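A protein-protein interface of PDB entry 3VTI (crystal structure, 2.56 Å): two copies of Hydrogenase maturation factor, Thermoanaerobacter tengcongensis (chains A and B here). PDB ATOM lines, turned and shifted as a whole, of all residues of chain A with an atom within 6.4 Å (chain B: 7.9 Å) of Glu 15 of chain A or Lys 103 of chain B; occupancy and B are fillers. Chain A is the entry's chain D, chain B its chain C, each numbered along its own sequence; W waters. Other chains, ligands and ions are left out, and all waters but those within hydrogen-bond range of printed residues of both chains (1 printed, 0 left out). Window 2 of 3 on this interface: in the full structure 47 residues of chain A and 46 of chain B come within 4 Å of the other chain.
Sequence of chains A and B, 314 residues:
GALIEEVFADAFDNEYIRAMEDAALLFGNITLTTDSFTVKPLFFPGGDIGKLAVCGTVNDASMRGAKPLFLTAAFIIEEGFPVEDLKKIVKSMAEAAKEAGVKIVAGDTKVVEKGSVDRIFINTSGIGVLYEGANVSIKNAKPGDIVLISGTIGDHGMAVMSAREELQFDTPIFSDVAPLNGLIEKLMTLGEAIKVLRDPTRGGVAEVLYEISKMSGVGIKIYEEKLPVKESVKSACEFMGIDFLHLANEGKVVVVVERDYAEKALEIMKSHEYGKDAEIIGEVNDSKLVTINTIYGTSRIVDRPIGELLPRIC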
ATOM      1  N   ASP A  13      16.873 -19.123  16.400  1.00  0.00           N
ATOM      2  CA  ASP A  13      17.214 -18.666  15.053  1.00  0.00           C
ATOM      3  C   ASP A  13      17.228 -19.824  14.052  1.00  0.00           C
ATOM      4  O   ASP A  13      18.076 -20.719  14.113  1.00  0.00           O
ATOM      5  CB  ASP A  13      18.529 -17.856  15.026  1.00  0.00           C
ATOM      6  CG  ASP A  13      19.747 -18.650  15.515  1.00  0.00           C
ATOM      7  OD1 ASP A  13      19.601 -19.558  16.366  1.00  0.00           O
ATOM      8  OD2 ASP A  13      20.869 -18.353  15.050  1.00  0.00           O
ATOM      9  N   ASN A  14      16.245 -19.799  13.157  1.00  0.00           N
ATOM     10  CA  ASN A  14      16.142 -20.721  12.026  1.00  0.00           C
ATOM     11  C   ASN A  14      15.497 -19.995  10.838  1.00  0.00           C
ATOM     12  O   ASN A  14      15.213 -18.799  10.928  1.00  0.00           O
ATOM     13  CB  ASN A  14      15.374 -22.006  12.410  1.00  0.00           C
ATOM     14  CG  ASN A  14      14.026 -21.729  13.087  1.00  0.00           C
ATOM     15  OD1 ASN A  14      13.123 -21.132  12.497  1.00  0.00           O
ATOM     16  ND2 ASN A  14      13.887 -22.186  14.325  1.00  0.00           N
ATOM     17  N   GLU A  15      15.271 -20.709   9.736  1.00  0.00           N
ATOM     18  CA  GLU A  15      14.659 -20.130   8.527  1.00  0.00           C
ATOM     19  C   GLU A  15      13.179 -19.719   8.691  1.00  0.00           C
ATOM     20  O   GLU A  15      12.710 -18.792   8.019  1.00  0.00           O
ATOM     21  CB  GLU A  15      14.841 -21.069   7.316  1.00  0.00           C
ATOM     22  CG  GLU A  15      14.298 -22.501   7.499  1.00  0.00           C
ATOM     23  CD  GLU A  15      15.316 -23.490   8.087  1.00  0.00           C
ATOM     24  OE1 GLU A  15      15.997 -23.173   9.093  1.00  0.00           O
ATOM     25  OE2 GLU A  15      15.425 -24.609   7.539  1.00  0.00           O
ATOM     26  N   TYR A  16      12.458 -20.404   9.584  1.00  0.00           N
ATOM     27  CA  TYR A  16      11.026 -20.143   9.826  1.00  0.00           C
ATOM     28  C   TYR A  16      10.796 -18.962  10.776  1.00  0.00           C
ATOM     29  O   TYR A  16       9.929 -18.111  10.527  1.00  0.00           O
ATOM     30  CB  TYR A  16      10.316 -21.383  10.386  1.00  0.00           C
ATOM     31  CG  TYR A  16      10.375 -22.626   9.520  1.00  0.00           C
ATOM     32  CD1 TYR A  16       9.384 -22.891   8.573  1.00  0.00           C
ATOM     33  CD2 TYR A  16      11.409 -23.547   9.667  1.00  0.00           C
ATOM     34  CE1 TYR A  16       9.429 -24.038   7.783  1.00  0.00           C
ATOM     35  CE2 TYR A  16      11.465 -24.697   8.885  1.00  0.00           C
ATOM     36  CZ  TYR A  16      10.474 -24.938   7.945  1.00  0.00           C
ATOM     37  OH  TYR A  16      10.542 -26.078   7.171  1.00  0.00           O
ATOM     38  N   ILE A  17      11.565 -18.925  11.865  1.00  0.00           N
ATOM     39  CA  ILE A  17      11.481 -17.847  12.854  1.00  0.00           C
ATOM     40  C   ILE A  17      11.850 -16.488  12.247  1.00  0.00           C
ATOM     41  O   ILE A  17      11.091 -15.527  12.377  1.00  0.00           O
ATOM     42  CB  ILE A  17      12.358 -18.156  14.110  1.00  0.00           C
ATOM     43  CG1 ILE A  17      11.750 -19.304  14.930  1.00  0.00           C
ATOM     44  CG2 ILE A  17      12.593 -16.895  14.978  1.00  0.00           C
ATOM     45  CD1 ILE A  17      10.363 -19.027  15.509  1.00  0.00           C
ATOM     46  N   ARG A  18      13.003 -16.433  11.575  1.00  0.00           N
ATOM     47  CA  ARG A  18      13.526 -15.208  10.943  1.00  0.00           C
ATOM     48  C   ARG A  18      12.589 -14.576   9.905  1.00  0.00           C
ATOM     49  O   ARG A  18      12.728 -13.399   9.574  1.00  0.00           O
ATOM     50  CB  ARG A  18      14.883 -15.486  10.289  1.00  0.00           C
ATOM     51  CG  ARG A  18      16.042 -15.685  11.259  1.00  0.00           C
ATOM     52  CD  ARG A  18      17.262 -16.177  10.493  1.00  0.00           C
ATOM     53  NE  ARG A  18      18.537 -15.772  11.089  1.00  0.00           N
ATOM     54  CZ  ARG A  18      19.042 -14.537  11.043  1.00  0.00           C
ATOM     55  NH1 ARG A  18      18.370 -13.547  10.453  1.00  0.00           N
ATOM     56  NH2 ARG A  18      20.219 -14.285  11.606  1.00  0.00           N
ATOM     57  N   ALA A  19      11.651 -15.364   9.381  1.00  0.00           N
ATOM     58  CA  ALA A  19      10.676 -14.867   8.420  1.00  0.00           C
ATOM     59  C   ALA A  19       9.594 -14.017   9.089  1.00  0.00           C
ATOM     60  O   ALA A  19       8.944 -13.210   8.423  1.00  0.00           O
ATOM     61  CB  ALA A  19      10.064 -16.019   7.639  1.00  0.00           C
ATOM     62  N   MET A  20       9.418 -14.195  10.404  1.00  0.00           N
ATOM     63  CA  MET A  20       8.475 -13.405  11.230  1.00  0.00           C
ATOM     64  C   MET A  20       7.048 -13.360  10.659  1.00  0.00           C
ATOM     65  O   MET A  20       6.462 -12.291  10.481  1.00  0.00           O
ATOM     66  CB  MET A  20       9.009 -11.990  11.469  1.00  0.00           C
ATOM     67  CG  MET A  20      10.301 -11.931  12.246  1.00  0.00           C
ATOM     68  SD  MET A  20      10.709 -10.246  12.746  1.00  0.00           S
ATOM     69  CE  MET A  20      12.003 -10.544  13.966  1.00  0.00           C
ATOM     70  N   LYS A 139       6.937 -10.895   3.257  1.00  0.00           N
ATOM     71  CA  LYS A 139       8.055 -10.474   2.419  1.00  0.00           C
ATOM     72  C   LYS A 139       7.622 -10.122   1.002  1.00  0.00           C
ATOM     73  O   LYS A 139       8.410  -9.574   0.227  1.00  0.00           O
ATOM     74  CB  LYS A 139       9.103 -11.585   2.346  1.00  0.00           C
ATOM     75  CG  LYS A 139      10.103 -11.605   3.489  1.00  0.00           C
ATOM     76  CD  LYS A 139      11.089 -12.765   3.373  1.00  0.00           C
ATOM     77  CE  LYS A 139      10.507 -14.059   3.917  1.00  0.00           C
ATOM     78  NZ  LYS A 139      11.357 -15.234   3.563  1.00  0.00           N
ATOM     79  N   VAL B  54       9.895 -28.475  26.038  1.00  0.00           N
ATOM     80  CA  VAL B  54      10.238 -29.059  24.750  1.00  0.00           C
ATOM     81  C   VAL B  54      10.017 -30.573  24.787  1.00  0.00           C
ATOM     82  O   VAL B  54       9.237 -31.106  24.007  1.00  0.00           O
ATOM     83  CB  VAL B  54      11.696 -28.741  24.332  1.00  0.00           C
ATOM     84  CG1 VAL B  54      12.029 -29.388  22.995  1.00  0.00           C
ATOM     85  CG2 VAL B  54      11.904 -27.240  24.249  1.00  0.00           C
ATOM     86  N   VAL B  58       7.648 -32.969  22.545  1.00  0.00           N
ATOM     87  CA  VAL B  58       8.344 -33.857  21.629  1.00  0.00           C
ATOM     88  C   VAL B  58       7.859 -35.281  21.896  1.00  0.00           C
ATOM     89  O   VAL B  58       7.538 -36.030  20.973  1.00  0.00           O
ATOM     90  CB  VAL B  58       9.888 -33.737  21.788  1.00  0.00           C
ATOM     91  CG1 VAL B  58      10.622 -34.954  21.173  1.00  0.00           C
ATOM     92  CG2 VAL B  58      10.395 -32.411  21.192  1.00  0.00           C
ATOM     93  N   PRO B  68       8.626 -36.461  15.628  1.00  0.00           N
ATOM     94  CA  PRO B  68       8.257 -35.060  15.796  1.00  0.00           C
ATOM     95  C   PRO B  68       9.211 -34.173  15.009  1.00  0.00           C
ATOM     96  O   PRO B  68      10.398 -34.479  14.938  1.00  0.00           O
ATOM     97  CB  PRO B  68       8.415 -34.836  17.303  1.00  0.00           C
ATOM     98  CG  PRO B  68       9.450 -35.802  17.719  1.00  0.00           C
ATOM     99  CD  PRO B  68       9.310 -37.001  16.817  1.00  0.00           C
ATOM    100  N   LEU B  69       8.695 -33.094  14.423  1.00  0.00           N
ATOM    101  CA  LEU B  69       9.498 -32.219  13.564  1.00  0.00           C
ATOM    102  C   LEU B  69       9.437 -30.744  13.957  1.00  0.00           C
ATOM    103  O   LEU B  69      10.467 -30.067  14.007  1.00  0.00           O
ATOM    104  CB  LEU B  69       9.077 -32.356  12.095  1.00  0.00           C
ATOM    105  CG  LEU B  69       9.323 -33.641  11.299  1.00  0.00           C
ATOM    106  CD1 LEU B  69       8.509 -33.611  10.005  1.00  0.00           C
ATOM    107  CD2 LEU B  69      10.813 -33.858  10.991  1.00  0.00           C
ATOM    108  N   PHE B  70       8.230 -30.248  14.215  1.00  0.00           N
ATOM    109  CA  PHE B  70       8.014 -28.820  14.411  1.00  0.00           C
ATOM    110  C   PHE B  70       7.266 -28.538  15.688  1.00  0.00           C
ATOM    111  O   PHE B  70       6.371 -29.300  16.080  1.00  0.00           O
ATOM    112  CB  PHE B  70       7.277 -28.213  13.220  1.00  0.00           C
ATOM    113  CG  PHE B  70       7.927 -28.516  11.896  1.00  0.00           C
ATOM    114  CD1 PHE B  70       9.202 -28.023  11.598  1.00  0.00           C
ATOM    115  CD2 PHE B  70       7.278 -29.309  10.952  1.00  0.00           C
ATOM    116  CE1 PHE B  70       9.811 -28.309  10.368  1.00  0.00           C
ATOM    117  CE2 PHE B  70       7.877 -29.592   9.722  1.00  0.00           C
ATOM    118  CZ  PHE B  70       9.144 -29.096   9.430  1.00  0.00           C
ATOM    119  N   LEU B  71       7.656 -27.441  16.336  1.00  0.00           N
ATOM    120  CA  LEU B  71       7.086 -27.034  17.607  1.00  0.00           C
ATOM    121  C   LEU B  71       6.744 -25.552  17.638  1.00  0.00           C
ATOM    122  O   LEU B  71       7.387 -24.732  16.980  1.00  0.00           O
ATOM    123  CB  LEU B  71       8.050 -27.355  18.751  1.00  0.00           C
ATOM    124  CG  LEU B  71       7.825 -28.636  19.559  1.00  0.00           C
ATOM    125  CD1 LEU B  71       8.273 -29.862  18.780  1.00  0.00           C
ATOM    126  CD2 LEU B  71       8.540 -28.550  20.900  1.00  0.00           C
ATOM    127  N   THR B  72       5.721 -25.215  18.409  1.00  0.00           N
ATOM    128  CA  THR B  72       5.438 -23.827  18.687  1.00  0.00           C
ATOM    129  C   THR B  72       5.775 -23.575  20.142  1.00  0.00           C
ATOM    130  O   THR B  72       5.710 -24.494  20.954  1.00  0.00           O
ATOM    131  CB  THR B  72       3.978 -23.499  18.439  1.00  0.00           C
ATOM    132  OG1 THR B  72       3.169 -24.438  19.141  1.00  0.00           O
ATOM    133  CG2 THR B  72       3.652 -23.574  16.936  1.00  0.00           C
ATOM    134  N   ALA B  73       6.162 -22.346  20.467  1.00  0.00           N
ATOM    135  CA  ALA B  73       6.497 -21.997  21.842  1.00  0.00           C
ATOM    136  C   ALA B  73       5.816 -20.700  22.258  1.00  0.00           C
ATOM    137  O   ALA B  73       6.082 -19.642  21.694  1.00  0.00           O
ATOM    138  CB  ALA B  73       8.008 -21.906  22.032  1.00  0.00           C
ATOM    139  N   ALA B  96      17.327 -28.731  23.903  1.00  0.00           N
ATOM    140  CA  ALA B  96      16.429 -29.880  23.839  1.00  0.00           C
ATOM    141  C   ALA B  96      15.873 -30.119  22.430  1.00  0.00           C
ATOM    142  O   ALA B  96      15.771 -31.267  21.986  1.00  0.00           O
ATOM    143  CB  ALA B  96      15.302 -29.730  24.844  1.00  0.00           C
ATOM    144  N   ALA B  97      15.523 -29.036  21.735  1.00  0.00           N
ATOM    145  CA  ALA B  97      15.043 -29.118  20.355  1.00  0.00           C
ATOM    146  C   ALA B  97      16.133 -29.660  19.437  1.00  0.00           C
ATOM    147  O   ALA B  97      15.857 -30.465  18.540  1.00  0.00           O
ATOM    148  CB  ALA B  97      14.559 -27.767  19.869  1.00  0.00           C
ATOM    149  N   LYS B  98      17.367 -29.229  19.683  1.00  0.00           N
ATOM    150  CA  LYS B  98      18.528 -29.686  18.932  1.00  0.00           C
ATOM    151  C   LYS B  98      18.755 -31.192  19.119  1.00  0.00           C
ATOM    152  O   LYS B  98      18.950 -31.907  18.145  1.00  0.00           O
ATOM    153  CB  LYS B  98      19.765 -28.895  19.359  1.00  0.00           C
ATOM    154  CG  LYS B  98      20.786 -28.685  18.258  1.00  0.00           C
ATOM    155  CD  LYS B  98      21.591 -27.404  18.490  1.00  0.00           C
ATOM    156  CE  LYS B  98      22.900 -27.686  19.210  1.00  0.00           C
ATOM    157  NZ  LYS B  98      23.941 -28.135  18.247  1.00  0.00           N
ATOM    158  N   ALA B 100      16.523 -33.391  20.213  1.00  0.00           N
ATOM    159  CA  ALA B 100      15.362 -34.070  19.649  1.00  0.00           C
ATOM    160  C   ALA B 100      15.307 -34.007  18.116  1.00  0.00           C
ATOM    161  O   ALA B 100      14.497 -34.690  17.503  1.00  0.00           O
ATOM    162  CB  ALA B 100      14.080 -33.522  20.257  1.00  0.00           C
ATOM    163  N   GLY B 101      16.168 -33.197  17.501  1.00  0.00           N
ATOM    164  CA  GLY B 101      16.173 -33.039  16.044  1.00  0.00           C
ATOM    165  C   GLY B 101      14.908 -32.355  15.558  1.00  0.00           C
ATOM    166  O   GLY B 101      14.375 -32.684  14.496  1.00  0.00           O
ATOM    167  N   VAL B 102      14.443 -31.393  16.352  1.00  0.00           N
ATOM    168  CA  VAL B 102      13.177 -30.715  16.156  1.00  0.00           C
ATOM    169  C   VAL B 102      13.433 -29.202  16.024  1.00  0.00           C
ATOM    170  O   VAL B 102      14.489 -28.705  16.445  1.00  0.00           O
ATOM    171  CB  VAL B 102      12.238 -31.051  17.347  1.00  0.00           C
ATOM    172  CG1 VAL B 102      11.926 -29.825  18.224  1.00  0.00           C
ATOM    173  CG2 VAL B 102      10.976 -31.720  16.861  1.00  0.00           C
ATOM    174  N   LYS B 103      12.491 -28.477  15.422  1.00  0.00           N
ATOM    175  CA  LYS B 103      12.623 -27.026  15.276  1.00  0.00           C
ATOM    176  C   LYS B 103      11.393 -26.267  15.749  1.00  0.00           C
ATOM    177  O   LYS B 103      10.263 -26.638  15.418  1.00  0.00           O
ATOM    178  CB  LYS B 103      12.914 -26.650  13.830  1.00  0.00           C
ATOM    179  CG  LYS B 103      14.348 -26.855  13.423  1.00  0.00           C
ATOM    180  CD  LYS B 103      14.515 -26.683  11.918  1.00  0.00           C
ATOM    181  CE  LYS B 103      15.980 -26.720  11.523  1.00  0.00           C
ATOM    182  NZ  LYS B 103      16.110 -26.787  10.044  1.00  0.00           N
ATOM    183  N   ILE B 104      11.623 -25.206  16.522  1.00  0.00           N
ATOM    184  CA  ILE B 104      10.549 -24.300  16.928  1.00  0.00           C
ATOM    185  C   ILE B 104      10.364 -23.267  15.831  1.00  0.00           C
ATOM    186  O   ILE B 104      11.273 -22.489  15.536  1.00  0.00           O
ATOM    187  CB  ILE B 104      10.829 -23.628  18.291  1.00  0.00           C
ATOM    188  CG1 ILE B 104      11.027 -24.700  19.368  1.00  0.00           C
ATOM    189  CG2 ILE B 104       9.697 -22.655  18.667  1.00  0.00           C
ATOM    190  CD1 ILE B 104      11.759 -24.228  20.570  1.00  0.00           C
ATOM    191  N   VAL B 105       9.177 -23.269  15.234  1.00  0.00           N
ATOM    192  CA  VAL B 105       8.934 -22.576  13.967  1.00  0.00           C
ATOM    193  C   VAL B 105       7.999 -21.386  14.085  1.00  0.00           C
ATOM    194  O   VAL B 105       7.988 -20.498  13.224  1.00  0.00           O
ATOM    195  CB  VAL B 105       8.396 -23.548  12.904  1.00  0.00           C
ATOM    196  CG1 VAL B 105       9.482 -24.554  12.523  1.00  0.00           C
ATOM    197  CG2 VAL B 105       7.145 -24.264  13.403  1.00  0.00           C
ATOM    198  N   ALA B 106       7.216 -21.380  15.154  1.00  0.00           N
ATOM    199  CA  ALA B 106       6.301 -20.286  15.455  1.00  0.00           C
ATOM    200  C   ALA B 106       6.237 -20.090  16.963  1.00  0.00           C
ATOM    201  O   ALA B 106       6.658 -20.951  17.736  1.00  0.00           O
ATOM    202  CB  ALA B 106       4.912 -20.582  14.907  1.00  0.00           C
ATOM    203  N   SER B 125       3.214 -26.461  21.417  1.00  0.00           N
ATOM    204  CA  SER B 125       2.500 -27.410  20.559  1.00  0.00           C
ATOM    205  C   SER B 125       3.483 -28.096  19.629  1.00  0.00           C
ATOM    206  O   SER B 125       4.572 -27.572  19.368  1.00  0.00           O
ATOM    207  CB  SER B 125       1.401 -26.722  19.750  1.00  0.00           C
ATOM    208  OG  SER B 125       0.531 -26.002  20.606  1.00  0.00           O
ATOM    209  N   GLY B 126       3.101 -29.260  19.121  1.00  0.00           N
ATOM    210  CA  GLY B 126       4.011 -30.049  18.318  1.00  0.00           C
ATOM    211  C   GLY B 126       3.351 -30.690  17.126  1.00  0.00           C
ATOM    212  O   GLY B 126       2.179 -31.070  17.191  1.00  0.00           O
ATOM    213  N   ILE B 127       4.117 -30.804  16.041  1.00  0.00           N
ATOM    214  CA  ILE B 127       3.709 -31.527  14.847  1.00  0.00           C
ATOM    215  C   ILE B 127       4.709 -32.640  14.576  1.00  0.00           C
ATOM    216  O   ILE B 127       5.917 -32.412  14.553  1.00  0.00           O
ATOM    217  CB  ILE B 127       3.555 -30.572  13.629  1.00  0.00           C
ATOM    218  CG1 ILE B 127       2.137 -30.028  13.585  1.00  0.00           C
ATOM    219  CG2 ILE B 127       3.852 -31.261  12.298  1.00  0.00           C
ATOM    220  CD1 ILE B 127       1.924 -29.003  12.519  1.00  0.00           C
HETATM  221  O   HOH W   1      14.327 -24.494  16.835  1.00  0.00           O
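Asp 13 of chain A touches none of the printed residues of chain B.
Of the printed residues of chain B, Asn 14 of chain A touches Ile 104.
Of the printed residues of chain B, Ile 17 of chain A touches Ile 104, Val 105 and Ala 106.
Ala 73 of chain B touches none of the printed residues of chain A.
Lys 103 of chain B touches just one residue of chain A: Glu 15.
Printed residues of chain A within 4 Å of Ile 104 of chain B: Asn 14 and Ile 17.
Of the printed residues of chain A, Val 105 of chain B touches Tyr 16 (3.6 Å) and Ile 17 (3.6 Å).
Of the printed residues of chain A, Ala 106 of chain B touches Ile 17 (3.9 Å).
The nearest residue of chain B that does not touch Glu 15 of chain A is Val 105 of chain B (6.9 Å).
Of the 21 printed residues of chain B, 5 touch a printed residue of chain A.
Hydrophobic or aromatic side chains of chain B within 4 Å of the printed part of chain A: Phe 70 and Val 105.
Hydrophobic or aromatic side chains of chain A that line the printed part of chain B: Tyr 16 and Ile 17.
Among the printed residues, Asp or Glu carboxylates within 4 Å of a Lys or Arg side-chain nitrogen of the other chain: Glu 15 of chain A with Lys 103 of chain B (3.4 Å).
The backbone carbonyl oxygen (O) of Ile 104 of chain B sits at hydrogen-bond distance from the side-chain amide nitrogen (ND2) of Asn 14 of chain A (2.9 Å).
The side-chain carboxylate of Glu 15 of chain A is in salt-bridge range of the side-chain amino group of Lys 103 of chain B, 3.4 Å away.
Among the printed residues, merely in contact across the chains: Ile 17 of chain A with Ile 104 of chain B, Tyr 16 of chain A with Val 105 of chain B, Ile 17 of chain A with Val 105 of chain B, Ile 17 of chain A with Ala 106 of chain B and Tyr 16 of chain A with Phe 70 of chain B.
Water W1 lies within hydrogen-bond range of N of Ile 104 of chain B (2.8 Å) and ND2 of Asn 14 of chain A (3.4 Å).
The backbone NH of Lys 103 of chain B lies within hydrogen-bond range of the backbone carbonyl oxygen of Leu 69 of chain B, 2.9 Å away.
The backbone NH of Ala 73 of chain B sits at hydrogen-bond distance from the backbone carbonyl oxygen of Ala 106 of chain B (3.1 Å).
The backbone carbonyl oxygen (O) of Leu 71 of chain B is in hydrogen-bond range of the backbone NH (N) of Val 105 of chain B, 2.9 Å away.
The backbone NH (N) of Tyr 16 of chain A sits at hydrogen-bond distance from the side-chain amide oxygen (OD1) of Asn 14 of chain A (3.1 Å).
N of Ile 17 of chain A lies within hydrogen-bond range of OD1 of Asn 14 of chain A (2.8 Å).
The backbone carbonyl oxygen (O) of Phe 70 of chain B is in hydrogen-bond range of the backbone NH (N) of Ile 127 of chain B (2.7 Å).
No position is printed for both chains.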
